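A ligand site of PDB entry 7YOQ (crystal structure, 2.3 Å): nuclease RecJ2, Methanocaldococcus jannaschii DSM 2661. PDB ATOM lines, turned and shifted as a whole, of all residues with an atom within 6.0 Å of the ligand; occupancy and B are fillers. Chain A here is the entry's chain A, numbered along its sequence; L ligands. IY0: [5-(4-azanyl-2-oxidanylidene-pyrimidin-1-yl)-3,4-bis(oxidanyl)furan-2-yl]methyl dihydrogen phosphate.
N4 of the ligand sits close to O of Gly 400.
An oxygen (O17) of the ligand sits close to the backbone carbonyl oxygen of Ser 406 (3.5 Å).
CE1 of His 61 touches N7 of the ligand, 3.6 Å away.
O of Phe 370 touches O20 of the ligand, at 3.9 Å.
ND2 of Asn 398 touches N7 of the ligand (3.7 Å).
Gly 399 touches the ligand.
Gly 401 touches the ligand.
Ala 405 touches the ligand (O to C16, 3.6 Å).
N of Gly 407 touches O17 of the ligand, at 3.6 Å.
Of the 25 residues printed, 13 come within 4 Å of the ligand.
The nearest printed residue that does not touch the ligand is His 31 (4.01 Å).
OG of Ser 371 sits at hydrogen-bond distance from O20 of the ligand.
An oxygen (O14) of the ligand sits at hydrogen-bond distance from a ring nitrogen (NE2) of His 107.
NH2 of Arg 373 lies within salt-bridge range of O19 of the ligand, at 3.3 Å.
An oxygen (O21) of the ligand lies within salt-bridge range of the side-chain amino group (NZ) of Lys 369, 3.5 Å away.
O of Gly 400 sits close to OG of Ser 406 (3.4 Å).
The backbone carbonyl oxygen (O) of Gly 400 lies within hydrogen-bond range of the backbone NH (N) of Gly 407 (2.9 Å).
O of Ser 406 lies within hydrogen-bond range of NH1 of Arg 373, at 3.3 Å.
The backbone NH (N) of Gly 401 sits close to the side-chain hydroxyl (OG) of Ser 406.
The side-chain hydroxyl (OG) of Ser 406 lies within hydrogen-bond range of the backbone carbonyl oxygen (O) of His 402 (2.8 Å).
The backbone NH (N) of Ala 372 sits at hydrogen-bond distance from the backbone carbonyl oxygen (O) of Ser 406, 2.9 Å away.
ND2 of Asn 398 sits at hydrogen-bond distance from NE2 of His 61 (3.3 Å).
The backbone NH of Phe 370 lies within hydrogen-bond range of the backbone carbonyl oxygen of Ala 408, at 2.8 Å.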
ATOM      1  N   HIS A  31     -15.542 -11.486  21.149  1.00  0.00           N
ATOM      2  CA  HIS A  31     -14.933 -10.204  21.409  1.00  0.00           C
ATOM      3  C   HIS A  31     -13.724 -10.392  22.309  1.00  0.00           C
ATOM      4  O   HIS A  31     -13.574 -11.429  22.971  1.00  0.00           O
ATOM      5  CB  HIS A  31     -15.953  -9.248  22.036  1.00  0.00           C
ATOM      6  CG  HIS A  31     -15.657  -7.805  21.800  1.00  0.00           C
ATOM      7  ND1 HIS A  31     -15.851  -6.829  22.751  1.00  0.00           N
ATOM      8  CD2 HIS A  31     -15.136  -7.175  20.715  1.00  0.00           C
ATOM      9  CE1 HIS A  31     -15.498  -5.653  22.260  1.00  0.00           C
ATOM     10  NE2 HIS A  31     -15.052  -5.840  21.024  1.00  0.00           N
ATOM     11  N   HIS A  32     -12.879  -9.359  22.362  1.00  0.00           N
ATOM     12  CA  HIS A  32     -11.624  -9.405  23.089  1.00  0.00           C
ATOM     13  C   HIS A  32     -11.723  -8.849  24.506  1.00  0.00           C
ATOM     14  O   HIS A  32     -10.700  -8.804  25.210  1.00  0.00           O
ATOM     15  CB  HIS A  32     -10.520  -8.672  22.289  1.00  0.00           C
ATOM     16  CG  HIS A  32     -10.657  -7.175  22.292  1.00  0.00           C
ATOM     17  ND1 HIS A  32     -11.777  -6.528  21.811  1.00  0.00           N
ATOM     18  CD2 HIS A  32      -9.814  -6.197  22.696  1.00  0.00           C
ATOM     19  CE1 HIS A  32     -11.615  -5.223  21.941  1.00  0.00           C
ATOM     20  NE2 HIS A  32     -10.431  -4.995  22.467  1.00  0.00           N
ATOM     21  N   ASP A  33     -12.911  -8.449  24.955  1.00  0.00           N
ATOM     22  CA  ASP A  33     -13.016  -7.985  26.325  1.00  0.00           C
ATOM     23  C   ASP A  33     -13.173  -9.173  27.299  1.00  0.00           C
ATOM     24  O   ASP A  33     -13.240 -10.341  26.901  1.00  0.00           O
ATOM     25  CB  ASP A  33     -14.182  -6.991  26.450  1.00  0.00           C
ATOM     26  CG  ASP A  33     -15.562  -7.648  26.242  1.00  0.00           C
ATOM     27  OD1 ASP A  33     -15.704  -8.560  25.388  1.00  0.00           O
ATOM     28  OD2 ASP A  33     -16.505  -7.254  26.949  1.00  0.00           O
ATOM     29  N   GLU A  60     -11.743  -7.609  17.393  1.00  0.00           N
ATOM     30  CA  GLU A  60     -12.002  -6.398  18.171  1.00  0.00           C
ATOM     31  C   GLU A  60     -13.375  -5.816  17.843  1.00  0.00           C
ATOM     32  O   GLU A  60     -14.090  -5.342  18.738  1.00  0.00           O
ATOM     33  CB  GLU A  60     -10.893  -5.381  17.936  1.00  0.00           C
ATOM     34  CG  GLU A  60      -9.624  -5.636  18.766  1.00  0.00           C
ATOM     35  CD  GLU A  60      -8.351  -5.137  18.103  1.00  0.00           C
ATOM     36  OE1 GLU A  60      -7.337  -5.888  18.080  1.00  0.00           O
ATOM     37  OE2 GLU A  60      -8.353  -3.981  17.597  1.00  0.00           O
ATOM     38  N   HIS A  61     -13.764  -5.852  16.569  1.00  0.00           N
ATOM     39  CA  HIS A  61     -15.067  -5.382  16.147  1.00  0.00           C
ATOM     40  C   HIS A  61     -15.578  -6.242  14.995  1.00  0.00           C
ATOM     41  O   HIS A  61     -14.806  -6.629  14.115  1.00  0.00           O
ATOM     42  CB  HIS A  61     -15.010  -3.912  15.709  1.00  0.00           C
ATOM     43  CG  HIS A  61     -16.334  -3.406  15.230  1.00  0.00           C
ATOM     44  ND1 HIS A  61     -17.526  -3.765  15.821  1.00  0.00           N
ATOM     45  CD2 HIS A  61     -16.645  -2.585  14.196  1.00  0.00           C
ATOM     46  CE1 HIS A  61     -18.519  -3.189  15.185  1.00  0.00           C
ATOM     47  NE2 HIS A  61     -18.014  -2.469  14.194  1.00  0.00           N
ATOM     48  N   ASP A  85     -21.208 -12.422  22.100  1.00  0.00           N
ATOM     49  CA  ASP A  85     -21.004 -11.011  22.458  1.00  0.00           C
ATOM     50  C   ASP A  85     -21.035 -10.102  21.235  1.00  0.00           C
ATOM     51  O   ASP A  85     -20.401  -9.030  21.243  1.00  0.00           O
ATOM     52  CB  ASP A  85     -19.689 -10.817  23.228  1.00  0.00           C
ATOM     53  N   MET A  86     -21.759 -10.485  20.186  1.00  0.00           N
ATOM     54  CA  MET A  86     -21.759  -9.760  18.912  1.00  0.00           C
ATOM     55  C   MET A  86     -22.732 -10.488  17.994  1.00  0.00           C
ATOM     56  O   MET A  86     -23.173 -11.601  18.298  1.00  0.00           O
ATOM     57  CB  MET A  86     -20.382  -9.688  18.262  1.00  0.00           C
ATOM     58  CG  MET A  86     -19.838 -11.043  17.836  1.00  0.00           C
ATOM     59  SD  MET A  86     -18.234 -10.961  16.992  1.00  0.00           S
ATOM     60  CE  MET A  86     -17.231 -10.313  18.353  1.00  0.00           C
ATOM     61  N   GLN A  90     -25.235  -6.578  13.904  1.00  0.00           N
ATOM     62  CA  GLN A  90     -24.815  -6.880  12.536  1.00  0.00           C
ATOM     63  C   GLN A  90     -25.707  -7.940  11.878  1.00  0.00           C
ATOM     64  O   GLN A  90     -25.287  -8.570  10.907  1.00  0.00           O
ATOM     65  CB  GLN A  90     -23.348  -7.341  12.533  1.00  0.00           C
ATOM     66  CG  GLN A  90     -22.334  -6.368  13.191  1.00  0.00           C
ATOM     67  CD  GLN A  90     -22.269  -6.423  14.745  1.00  0.00           C
ATOM     68  OE1 GLN A  90     -22.887  -7.285  15.393  1.00  0.00           O
ATOM     69  NE2 GLN A  90     -21.484  -5.522  15.329  1.00  0.00           N
ATOM     70  N   HIS A 107     -26.232  -7.348  23.342  1.00  0.00           N
ATOM     71  CA  HIS A 107     -26.438  -5.990  22.847  1.00  0.00           C
ATOM     72  C   HIS A 107     -27.863  -5.824  22.323  1.00  0.00           C
ATOM     73  O   HIS A 107     -28.508  -6.806  21.960  1.00  0.00           O
ATOM     74  CB  HIS A 107     -25.433  -5.681  21.734  1.00  0.00           C
ATOM     75  CG  HIS A 107     -24.015  -5.609  22.222  1.00  0.00           C
ATOM     76  ND1 HIS A 107     -23.195  -6.716  22.309  1.00  0.00           N
ATOM     77  CD2 HIS A 107     -23.289  -4.566  22.687  1.00  0.00           C
ATOM     78  CE1 HIS A 107     -22.021  -6.359  22.783  1.00  0.00           C
ATOM     79  NE2 HIS A 107     -22.048  -5.060  23.027  1.00  0.00           N
ATOM     80  N   ARG A 288      -6.421  -6.603  26.250  1.00  0.00           N
ATOM     81  CA  ARG A 288      -6.017  -5.274  25.789  1.00  0.00           C
ATOM     82  C   ARG A 288      -4.618  -5.294  25.203  1.00  0.00           C
ATOM     83  O   ARG A 288      -4.278  -4.420  24.406  1.00  0.00           O
ATOM     84  CB  ARG A 288      -6.094  -4.267  26.946  1.00  0.00           C
ATOM     85  CG  ARG A 288      -7.499  -4.082  27.487  1.00  0.00           C
ATOM     86  CD  ARG A 288      -8.481  -3.657  26.382  1.00  0.00           C
ATOM     87  NE  ARG A 288      -9.862  -3.919  26.765  1.00  0.00           N
ATOM     88  CZ  ARG A 288     -10.939  -3.541  26.081  1.00  0.00           C
ATOM     89  NH1 ARG A 288     -10.823  -2.858  24.940  1.00  0.00           N
ATOM     90  NH2 ARG A 288     -12.148  -3.845  26.542  1.00  0.00           N
ATOM     91  N   GLY A 346     -11.180   2.710  26.874  1.00  0.00           N
ATOM     92  CA  GLY A 346     -12.442   2.320  27.494  1.00  0.00           C
ATOM     93  C   GLY A 346     -12.376   2.317  29.007  1.00  0.00           C
ATOM     94  O   GLY A 346     -13.288   2.786  29.683  1.00  0.00           O
ATOM     95  N   LYS A 369     -10.988   5.710  16.806  1.00  0.00           N
ATOM     96  CA  LYS A 369     -11.883   4.808  17.521  1.00  0.00           C
ATOM     97  C   LYS A 369     -12.300   5.460  18.828  1.00  0.00           C
ATOM     98  O   LYS A 369     -11.450   5.967  19.571  1.00  0.00           O
ATOM     99  CB  LYS A 369     -11.186   3.467  17.777  1.00  0.00           C
ATOM    100  CG  LYS A 369     -12.096   2.307  18.197  1.00  0.00           C
ATOM    101  CD  LYS A 369     -12.016   2.024  19.694  1.00  0.00           C
ATOM    102  CE  LYS A 369     -13.201   1.192  20.152  1.00  0.00           C
ATOM    103  NZ  LYS A 369     -14.464   1.943  19.924  1.00  0.00           N
ATOM    104  N   PHE A 370     -13.602   5.455  19.113  1.00  0.00           N
ATOM    105  CA  PHE A 370     -14.139   6.113  20.297  1.00  0.00           C
ATOM    106  C   PHE A 370     -14.752   5.095  21.233  1.00  0.00           C
ATOM    107  O   PHE A 370     -15.409   4.145  20.783  1.00  0.00           O
ATOM    108  CB  PHE A 370     -15.190   7.158  19.926  1.00  0.00           C
ATOM    109  CG  PHE A 370     -14.640   8.320  19.167  1.00  0.00           C
ATOM    110  CD1 PHE A 370     -14.307   8.185  17.826  1.00  0.00           C
ATOM    111  CD2 PHE A 370     -14.449   9.537  19.793  1.00  0.00           C
ATOM    112  CE1 PHE A 370     -13.783   9.254  17.112  1.00  0.00           C
ATOM    113  CE2 PHE A 370     -13.934  10.621  19.088  1.00  0.00           C
ATOM    114  CZ  PHE A 370     -13.597  10.478  17.742  1.00  0.00           C
ATOM    115  N   SER A 371     -14.552   5.278  22.536  1.00  0.00           N
ATOM    116  CA  SER A 371     -15.185   4.472  23.573  1.00  0.00           C
ATOM    117  C   SER A 371     -15.900   5.404  24.544  1.00  0.00           C
ATOM    118  O   SER A 371     -15.250   6.148  25.288  1.00  0.00           O
ATOM    119  CB  SER A 371     -14.181   3.595  24.310  1.00  0.00           C
ATOM    120  OG  SER A 371     -13.712   2.540  23.488  1.00  0.00           O
ATOM    121  N   ALA A 372     -17.228   5.363  24.541  1.00  0.00           N
ATOM    122  CA  ALA A 372     -18.046   6.230  25.375  1.00  0.00           C
ATOM    123  C   ALA A 372     -18.577   5.450  26.571  1.00  0.00           C
ATOM    124  O   ALA A 372     -19.094   4.337  26.417  1.00  0.00           O
ATOM    125  CB  ALA A 372     -19.214   6.806  24.557  1.00  0.00           C
ATOM    126  N   ARG A 373     -18.460   6.032  27.756  1.00  0.00           N
ATOM    127  CA  ARG A 373     -18.944   5.397  28.971  1.00  0.00           C
ATOM    128  C   ARG A 373     -19.872   6.339  29.727  1.00  0.00           C
ATOM    129  O   ARG A 373     -19.617   7.553  29.814  1.00  0.00           O
ATOM    130  CB  ARG A 373     -17.780   4.974  29.875  1.00  0.00           C
ATOM    131  CG  ARG A 373     -16.845   3.925  29.239  1.00  0.00           C
ATOM    132  CD  ARG A 373     -17.577   2.651  28.808  1.00  0.00           C
ATOM    133  NE  ARG A 373     -16.655   1.668  28.244  1.00  0.00           N
ATOM    134  CZ  ARG A 373     -16.434   1.475  26.939  1.00  0.00           C
ATOM    135  NH1 ARG A 373     -17.082   2.194  26.042  1.00  0.00           N
ATOM    136  NH2 ARG A 373     -15.569   0.558  26.556  1.00  0.00           N
ATOM    137  N   ASN A 398     -19.450   3.850  11.586  1.00  0.00           N
ATOM    138  CA  ASN A 398     -20.547   3.232  12.331  1.00  0.00           C
ATOM    139  C   ASN A 398     -20.208   3.222  13.806  1.00  0.00           C
ATOM    140  O   ASN A 398     -19.043   3.306  14.209  1.00  0.00           O
ATOM    141  CB  ASN A 398     -20.842   1.803  11.831  1.00  0.00           C
ATOM    142  CG  ASN A 398     -19.740   0.826  12.178  1.00  0.00           C
ATOM    143  OD1 ASN A 398     -18.569   1.089  11.901  1.00  0.00           O
ATOM    144  ND2 ASN A 398     -20.099  -0.306  12.786  1.00  0.00           N
ATOM    145  N   GLY A 399     -21.263   3.145  14.613  1.00  0.00           N
ATOM    146  CA  GLY A 399     -21.115   3.039  16.049  1.00  0.00           C
ATOM    147  C   GLY A 399     -22.277   2.287  16.633  1.00  0.00           C
ATOM    148  O   GLY A 399     -23.333   2.144  15.998  1.00  0.00           O
ATOM    149  N   GLY A 400     -22.085   1.796  17.846  1.00  0.00           N
ATOM    150  CA  GLY A 400     -23.136   1.095  18.557  1.00  0.00           C
ATOM    151  C   GLY A 400     -22.618   0.535  19.866  1.00  0.00           C
ATOM    152  O   GLY A 400     -21.450   0.699  20.224  1.00  0.00           O
ATOM    153  N   GLY A 401     -23.512  -0.142  20.552  1.00  0.00           N
ATOM    154  CA  GLY A 401     -23.183  -0.800  21.805  1.00  0.00           C
ATOM    155  C   GLY A 401     -24.387  -0.825  22.732  1.00  0.00           C
ATOM    156  O   GLY A 401     -25.513  -0.993  22.289  1.00  0.00           O
ATOM    157  N   HIS A 402     -24.101  -0.693  24.029  1.00  0.00           N
ATOM    158  CA  HIS A 402     -25.125  -0.614  25.057  1.00  0.00           C
ATOM    159  C   HIS A 402     -25.474   0.837  25.353  1.00  0.00           C
ATOM    160  O   HIS A 402     -24.699   1.767  25.083  1.00  0.00           O
ATOM    161  CB  HIS A 402     -24.673  -1.287  26.365  1.00  0.00           C
ATOM    162  CG  HIS A 402     -24.197  -2.699  26.211  1.00  0.00           C
ATOM    163  ND1 HIS A 402     -22.853  -3.043  26.223  1.00  0.00           N
ATOM    164  CD2 HIS A 402     -24.867  -3.870  26.097  1.00  0.00           C
ATOM    165  CE1 HIS A 402     -22.734  -4.355  26.108  1.00  0.00           C
ATOM    166  NE2 HIS A 402     -23.944  -4.877  26.025  1.00  0.00           N
ATOM    167  N   ALA A 405     -22.652   1.921  27.462  1.00  0.00           N
ATOM    168  CA  ALA A 405     -21.285   1.818  26.944  1.00  0.00           C
ATOM    169  C   ALA A 405     -21.310   1.448  25.468  1.00  0.00           C
ATOM    170  O   ALA A 405     -21.861   0.402  25.106  1.00  0.00           O
ATOM    171  CB  ALA A 405     -20.469   0.772  27.745  1.00  0.00           C
ATOM    172  N   SER A 406     -20.698   2.287  24.636  1.00  0.00           N
ATOM    173  CA  SER A 406     -20.728   2.114  23.194  1.00  0.00           C
ATOM    174  C   SER A 406     -19.405   2.555  22.588  1.00  0.00           C
ATOM    175  O   SER A 406     -18.560   3.153  23.260  1.00  0.00           O
ATOM    176  CB  SER A 406     -21.893   2.891  22.560  1.00  0.00           C
ATOM    177  OG  SER A 406     -23.110   2.206  22.765  1.00  0.00           O
ATOM    178  N   GLY A 407     -19.218   2.237  21.309  1.00  0.00           N
ATOM    179  CA  GLY A 407     -18.017   2.601  20.589  1.00  0.00           C
ATOM    180  C   GLY A 407     -18.372   3.145  19.221  1.00  0.00           C
ATOM    181  O   GLY A 407     -19.538   3.147  18.824  1.00  0.00           O
ATOM    182  N   ALA A 408     -17.350   3.595  18.494  1.00  0.00           N
ATOM    183  CA  ALA A 408     -17.548   4.150  17.167  1.00  0.00           C
ATOM    184  C   ALA A 408     -16.201   4.318  16.480  1.00  0.00           C
ATOM    185  O   ALA A 408     -15.154   4.320  17.127  1.00  0.00           O
ATOM    186  CB  ALA A 408     -18.290   5.496  17.229  1.00  0.00           C
HETATM  187  C13 IY0 L   1     -19.369  -3.641  22.051  1.00  0.00           C
HETATM  188  C1  IY0 L   1     -20.623  -1.234  17.642  1.00  0.00           C
HETATM  189  C2  IY0 L   1     -21.588  -1.998  18.365  1.00  0.00           C
HETATM  190  C3  IY0 L   1     -21.326  -2.469  19.632  1.00  0.00           C
HETATM  191  C5  IY0 L   1     -19.282  -1.367  19.329  1.00  0.00           C
HETATM  192  C9  IY0 L   1     -19.723  -2.502  21.395  1.00  0.00           C
HETATM  193  C11 IY0 L   1     -19.020  -1.880  23.275  1.00  0.00           C
HETATM  194  C12 IY0 L   1     -18.955  -3.235  23.268  1.00  0.00           C
HETATM  195  C16 IY0 L   1     -18.591  -0.885  24.191  1.00  0.00           C
HETATM  196  N4  IY0 L   1     -20.134  -2.156  20.154  1.00  0.00           N
HETATM  197  N6  IY0 L   1     -19.513  -0.922  18.090  1.00  0.00           N
HETATM  198  N7  IY0 L   1     -20.796  -0.734  16.388  1.00  0.00           N
HETATM  199  O8  IY0 L   1     -18.171  -1.030  19.756  1.00  0.00           O
HETATM  200  O10 IY0 L   1     -19.448  -1.527  22.137  1.00  0.00           O
HETATM  201  O14 IY0 L   1     -19.516  -4.868  21.633  1.00  0.00           O
HETATM  202  O15 IY0 L   1     -18.595  -4.031  24.219  1.00  0.00           O
HETATM  203  O17 IY0 L   1     -17.714  -0.194  23.443  1.00  0.00           O
HETATM  204  O19 IY0 L   1     -15.357  -1.316  23.843  1.00  0.00           O
HETATM  205  O20 IY0 L   1     -15.564   1.038  23.216  1.00  0.00           O
HETATM  206  O21 IY0 L   1     -16.038  -0.677  21.561  1.00  0.00           O
HETATM  207  P18 IY0 L   1     -15.948  -0.325  22.954  1.00  0.00           P
